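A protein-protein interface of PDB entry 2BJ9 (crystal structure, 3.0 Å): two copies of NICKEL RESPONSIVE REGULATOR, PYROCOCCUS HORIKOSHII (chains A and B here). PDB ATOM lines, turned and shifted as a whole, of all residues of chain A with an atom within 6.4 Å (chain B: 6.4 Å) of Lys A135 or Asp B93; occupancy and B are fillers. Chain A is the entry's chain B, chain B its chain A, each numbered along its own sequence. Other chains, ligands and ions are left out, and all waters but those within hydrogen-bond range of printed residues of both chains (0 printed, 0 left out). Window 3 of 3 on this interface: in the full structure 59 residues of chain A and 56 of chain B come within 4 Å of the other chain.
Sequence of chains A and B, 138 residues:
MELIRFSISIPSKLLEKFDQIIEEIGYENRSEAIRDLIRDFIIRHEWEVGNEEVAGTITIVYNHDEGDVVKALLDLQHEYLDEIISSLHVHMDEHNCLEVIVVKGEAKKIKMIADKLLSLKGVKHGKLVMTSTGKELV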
ATOM      1  N   GLU A  53      -8.324 -14.975   7.403  1.00  0.00           N
ATOM      2  CA  GLU A  53      -8.553 -14.453   8.736  1.00  0.00           C
ATOM      3  C   GLU A  53      -8.095 -15.387   9.846  1.00  0.00           C
ATOM      4  O   GLU A  53      -8.495 -16.545   9.905  1.00  0.00           O
ATOM      5  CB  GLU A  53     -10.043 -14.137   8.918  1.00  0.00           C
ATOM      6  CG  GLU A  53     -10.339 -12.966   9.856  1.00  0.00           C
ATOM      7  CD  GLU A  53     -10.448 -11.631   9.128  1.00  0.00           C
ATOM      8  OE1 GLU A  53      -9.616 -11.363   8.232  1.00  0.00           O
ATOM      9  OE2 GLU A  53     -11.364 -10.845   9.463  1.00  0.00           O
ATOM     10  N   LYS A 104      -7.176  -9.784  15.216  1.00  0.00           N
ATOM     11  CA  LYS A 104      -7.919 -10.593  14.263  1.00  0.00           C
ATOM     12  C   LYS A 104      -7.732 -10.003  12.873  1.00  0.00           C
ATOM     13  O   LYS A 104      -7.975  -8.822  12.667  1.00  0.00           O
ATOM     14  CB  LYS A 104      -9.405 -10.596  14.626  1.00  0.00           C
ATOM     15  CG  LYS A 104     -10.257 -11.522  13.779  1.00  0.00           C
ATOM     16  CD  LYS A 104     -11.724 -11.405  14.154  1.00  0.00           C
ATOM     17  CE  LYS A 104     -12.598 -12.258  13.248  1.00  0.00           C
ATOM     18  NZ  LYS A 104     -14.041 -12.152  13.616  1.00  0.00           N
ATOM     19  N   SER A 132      -6.588 -19.490  16.433  1.00  0.00           N
ATOM     20  CA  SER A 132      -7.578 -19.484  15.360  1.00  0.00           C
ATOM     21  C   SER A 132      -8.792 -18.634  15.676  1.00  0.00           C
ATOM     22  O   SER A 132      -8.887 -18.070  16.757  1.00  0.00           O
ATOM     23  CB  SER A 132      -8.027 -20.918  15.072  1.00  0.00           C
ATOM     24  OG  SER A 132      -8.854 -20.973  13.925  1.00  0.00           O
ATOM     25  N   THR A 133      -9.712 -18.541  14.720  1.00  0.00           N
ATOM     26  CA  THR A 133     -10.948 -17.780  14.900  1.00  0.00           C
ATOM     27  C   THR A 133     -12.088 -18.781  14.991  1.00  0.00           C
ATOM     28  O   THR A 133     -13.255 -18.403  15.023  1.00  0.00           O
ATOM     29  CB  THR A 133     -11.245 -16.855  13.711  1.00  0.00           C
ATOM     30  OG1 THR A 133     -11.542 -17.650  12.561  1.00  0.00           O
ATOM     31  CG2 THR A 133     -10.052 -15.963  13.409  1.00  0.00           C
ATOM     32  N   GLY A 134     -11.732 -20.063  15.009  1.00  0.00           N
ATOM     33  CA  GLY A 134     -12.723 -21.119  15.107  1.00  0.00           C
ATOM     34  C   GLY A 134     -13.487 -21.439  13.835  1.00  0.00           C
ATOM     35  O   GLY A 134     -13.757 -22.604  13.552  1.00  0.00           O
ATOM     36  N   LYS A 135     -13.830 -20.411  13.065  1.00  0.00           N
ATOM     37  CA  LYS A 135     -14.592 -20.572  11.830  1.00  0.00           C
ATOM     38  C   LYS A 135     -14.360 -21.863  11.039  1.00  0.00           C
ATOM     39  O   LYS A 135     -15.291 -22.387  10.426  1.00  0.00           O
ATOM     40  CB  LYS A 135     -14.362 -19.363  10.908  1.00  0.00           C
ATOM     41  CG  LYS A 135     -15.068 -19.463   9.551  1.00  0.00           C
ATOM     42  CD  LYS A 135     -14.919 -18.189   8.724  1.00  0.00           C
ATOM     43  CE  LYS A 135     -15.765 -17.045   9.278  1.00  0.00           C
ATOM     44  NZ  LYS A 135     -17.237 -17.294   9.162  1.00  0.00           N
ATOM     45  N   GLU A 136     -13.141 -22.388  11.053  1.00  0.00           N
ATOM     46  CA  GLU A 136     -12.866 -23.594  10.284  1.00  0.00           C
ATOM     47  C   GLU A 136     -12.380 -24.790  11.095  1.00  0.00           C
ATOM     48  O   GLU A 136     -11.796 -25.720  10.543  1.00  0.00           O
ATOM     49  CB  GLU A 136     -11.847 -23.277   9.189  1.00  0.00           C
ATOM     50  CG  GLU A 136     -10.411 -23.131   9.687  1.00  0.00           C
ATOM     51  CD  GLU A 136     -10.282 -22.192  10.872  1.00  0.00           C
ATOM     52  OE1 GLU A 136     -10.796 -21.056  10.795  1.00  0.00           O
ATOM     53  OE2 GLU A 136      -9.655 -22.588  11.880  1.00  0.00           O
ATOM     54  N   LEU A 137     -12.621 -24.776  12.400  1.00  0.00           N
ATOM     55  CA  LEU A 137     -12.186 -25.877  13.253  1.00  0.00           C
ATOM     56  C   LEU A 137     -13.353 -26.725  13.731  1.00  0.00           C
ATOM     57  O   LEU A 137     -14.515 -26.416  13.456  1.00  0.00           O
ATOM     58  CB  LEU A 137     -11.440 -25.341  14.478  1.00  0.00           C
ATOM     59  CG  LEU A 137     -10.067 -24.701  14.284  1.00  0.00           C
ATOM     60  CD1 LEU A 137      -9.609 -24.101  15.607  1.00  0.00           C
ATOM     61  CD2 LEU A 137      -9.074 -25.743  13.776  1.00  0.00           C
ATOM     62  N   HIS B  64     -18.599 -22.438  22.507  1.00  0.00           N
ATOM     63  CA  HIS B  64     -19.367 -22.368  23.741  1.00  0.00           C
ATOM     64  C   HIS B  64     -20.589 -23.267  23.724  1.00  0.00           C
ATOM     65  O   HIS B  64     -21.158 -23.570  24.772  1.00  0.00           O
ATOM     66  CB  HIS B  64     -19.800 -20.932  24.046  1.00  0.00           C
ATOM     67  CG  HIS B  64     -20.907 -20.440  23.174  1.00  0.00           C
ATOM     68  ND1 HIS B  64     -20.681 -19.843  21.953  1.00  0.00           N
ATOM     69  CD2 HIS B  64     -22.249 -20.476  23.336  1.00  0.00           C
ATOM     70  CE1 HIS B  64     -21.839 -19.530  21.401  1.00  0.00           C
ATOM     71  NE2 HIS B  64     -22.807 -19.904  22.219  1.00  0.00           N
ATOM     72  N   VAL B  90     -13.745 -12.535  23.661  1.00  0.00           N
ATOM     73  CA  VAL B  90     -14.164 -11.958  22.382  1.00  0.00           C
ATOM     74  C   VAL B  90     -14.995 -12.971  21.606  1.00  0.00           C
ATOM     75  O   VAL B  90     -14.492 -14.034  21.260  1.00  0.00           O
ATOM     76  CB  VAL B  90     -12.946 -11.594  21.527  1.00  0.00           C
ATOM     77  CG1 VAL B  90     -13.390 -11.044  20.177  1.00  0.00           C
ATOM     78  CG2 VAL B  90     -12.083 -10.588  22.274  1.00  0.00           C
ATOM     79  N   HIS B  91     -16.258 -12.648  21.331  1.00  0.00           N
ATOM     80  CA  HIS B  91     -17.126 -13.565  20.587  1.00  0.00           C
ATOM     81  C   HIS B  91     -16.732 -13.565  19.115  1.00  0.00           C
ATOM     82  O   HIS B  91     -17.008 -12.603  18.410  1.00  0.00           O
ATOM     83  CB  HIS B  91     -18.585 -13.139  20.717  1.00  0.00           C
ATOM     84  CG  HIS B  91     -19.027 -12.927  22.129  1.00  0.00           C
ATOM     85  ND1 HIS B  91     -18.996 -13.926  23.075  1.00  0.00           N
ATOM     86  CD2 HIS B  91     -19.499 -11.827  22.762  1.00  0.00           C
ATOM     87  CE1 HIS B  91     -19.429 -13.453  24.229  1.00  0.00           C
ATOM     88  NE2 HIS B  91     -19.740 -12.180  24.067  1.00  0.00           N
ATOM     89  N   MET B  92     -16.096 -14.645  18.661  1.00  0.00           N
ATOM     90  CA  MET B  92     -15.639 -14.771  17.276  1.00  0.00           C
ATOM     91  C   MET B  92     -16.745 -14.974  16.231  1.00  0.00           C
ATOM     92  O   MET B  92     -16.657 -14.450  15.122  1.00  0.00           O
ATOM     93  CB  MET B  92     -14.620 -15.902  17.179  1.00  0.00           C
ATOM     94  CG  MET B  92     -13.354 -15.655  17.983  1.00  0.00           C
ATOM     95  SD  MET B  92     -12.510 -14.120  17.533  1.00  0.00           S
ATOM     96  CE  MET B  92     -11.169 -14.741  16.609  1.00  0.00           C
ATOM     97  N   ASP B  93     -17.767 -15.750  16.572  1.00  0.00           N
ATOM     98  CA  ASP B  93     -18.893 -15.978  15.670  1.00  0.00           C
ATOM     99  C   ASP B  93     -20.045 -16.663  16.394  1.00  0.00           C
ATOM    100  O   ASP B  93     -20.067 -16.727  17.620  1.00  0.00           O
ATOM    101  CB  ASP B  93     -18.482 -16.789  14.430  1.00  0.00           C
ATOM    102  CG  ASP B  93     -18.031 -18.203  14.758  1.00  0.00           C
ATOM    103  OD1 ASP B  93     -18.748 -18.913  15.498  1.00  0.00           O
ATOM    104  OD2 ASP B  93     -16.962 -18.610  14.250  1.00  0.00           O
ATOM    105  N   GLU B  94     -21.008 -17.178  15.645  1.00  0.00           N
ATOM    106  CA  GLU B  94     -22.153 -17.813  16.274  1.00  0.00           C
ATOM    107  C   GLU B  94     -21.789 -18.798  17.381  1.00  0.00           C
ATOM    108  O   GLU B  94     -22.408 -18.790  18.444  1.00  0.00           O
ATOM    109  CB  GLU B  94     -23.010 -18.517  15.221  1.00  0.00           C
ATOM    110  CG  GLU B  94     -24.354 -19.019  15.743  1.00  0.00           C
ATOM    111  CD  GLU B  94     -25.243 -19.584  14.645  1.00  0.00           C
ATOM    112  OE1 GLU B  94     -26.394 -19.963  14.949  1.00  0.00           O
ATOM    113  OE2 GLU B  94     -24.799 -19.651  13.478  1.00  0.00           O
ATOM    114  N   HIS B  95     -20.773 -19.624  17.154  1.00  0.00           N
ATOM    115  CA  HIS B  95     -20.392 -20.638  18.135  1.00  0.00           C
ATOM    116  C   HIS B  95     -19.064 -20.441  18.851  1.00  0.00           C
ATOM    117  O   HIS B  95     -18.941 -20.728  20.043  1.00  0.00           O
ATOM    118  CB  HIS B  95     -20.353 -22.015  17.464  1.00  0.00           C
ATOM    119  CG  HIS B  95     -21.664 -22.455  16.890  1.00  0.00           C
ATOM    120  ND1 HIS B  95     -22.724 -22.852  17.674  1.00  0.00           N
ATOM    121  CD2 HIS B  95     -22.081 -22.568  15.606  1.00  0.00           C
ATOM    122  CE1 HIS B  95     -23.739 -23.191  16.899  1.00  0.00           C
ATOM    123  NE2 HIS B  95     -23.375 -23.028  15.639  1.00  0.00           N
ATOM    124  N   ASN B  96     -18.072 -19.957  18.124  1.00  0.00           N
ATOM    125  CA  ASN B  96     -16.738 -19.798  18.674  1.00  0.00           C
ATOM    126  C   ASN B  96     -16.415 -18.549  19.485  1.00  0.00           C
ATOM    127  O   ASN B  96     -16.829 -17.441  19.146  1.00  0.00           O
ATOM    128  CB  ASN B  96     -15.739 -19.959  17.534  1.00  0.00           C
ATOM    129  CG  ASN B  96     -15.944 -21.258  16.776  1.00  0.00           C
ATOM    130  OD1 ASN B  96     -15.819 -22.348  17.336  1.00  0.00           O
ATOM    131  ND2 ASN B  96     -16.276 -21.147  15.497  1.00  0.00           N
ATOM    132  N   CYS B  97     -15.664 -18.755  20.564  1.00  0.00           N
ATOM    133  CA  CYS B  97     -15.233 -17.679  21.450  1.00  0.00           C
ATOM    134  C   CYS B  97     -13.720 -17.737  21.568  1.00  0.00           C
ATOM    135  O   CYS B  97     -13.116 -18.786  21.368  1.00  0.00           O
ATOM    136  CB  CYS B  97     -15.809 -17.853  22.859  1.00  0.00           C
ATOM    137  SG  CYS B  97     -17.605 -17.914  23.016  1.00  0.00           S
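The side-chain hydroxyl (OG) of Ser A132 sits at hydrogen-bond distance from the backbone NH (N) of Gly A134, 3.2 Å away. The backbone NH (N) of Asn B96 is in hydrogen-bond range of the side-chain carboxylate (OD1) of Asp B93, 2.9 Å away. The side-chain carboxylate (OD1) of Asp B93 sits at hydrogen-bond distance from the backbone NH (N) of His B95 (2.7 Å).
Of the 8 printed residues of chain A, 4 touch a printed residue of chain B. Along chain A the printed residues that touch a printed residue of chain B span positions 104 to 135. Hydrophobic or aromatic side chains of chain B within 4 Å of the printed part of chain A: Met B92. Among the printed residues, 7 pairs touch across the chains.
Lys A104 touches Met B92. Met B92 touches Thr A133. Asp B93 touches Thr A133 (OD2 to O, 3.8 Å). O of Thr A133 touches CB of Asn B96 (3.9 Å). Gly A134 touches Asn B96. Lys A135 touches Asp B93. ND2 of Asn B96 touches N of Lys A135 (3.5 Å).
Lys A135 touches two residues of chain B. Printed residues of chain A within 4 Å of Asp B93: Thr A133 and Lys A135. Printed residues of chain B within 4 Å of Gly A134: Asn B96. Printed residues of chain B within 4 Å of Lys A104: Met B92 (3.8 Å). Cys B97 touches none of the printed residues of chain A. The nearest residue of chain B that does not touch Lys A135 is Met B92 (6.2 Å). The nearest residue of chain A that does not touch Asp B93 is Gly A134 (4.5 Å).
No position is printed for both chains.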
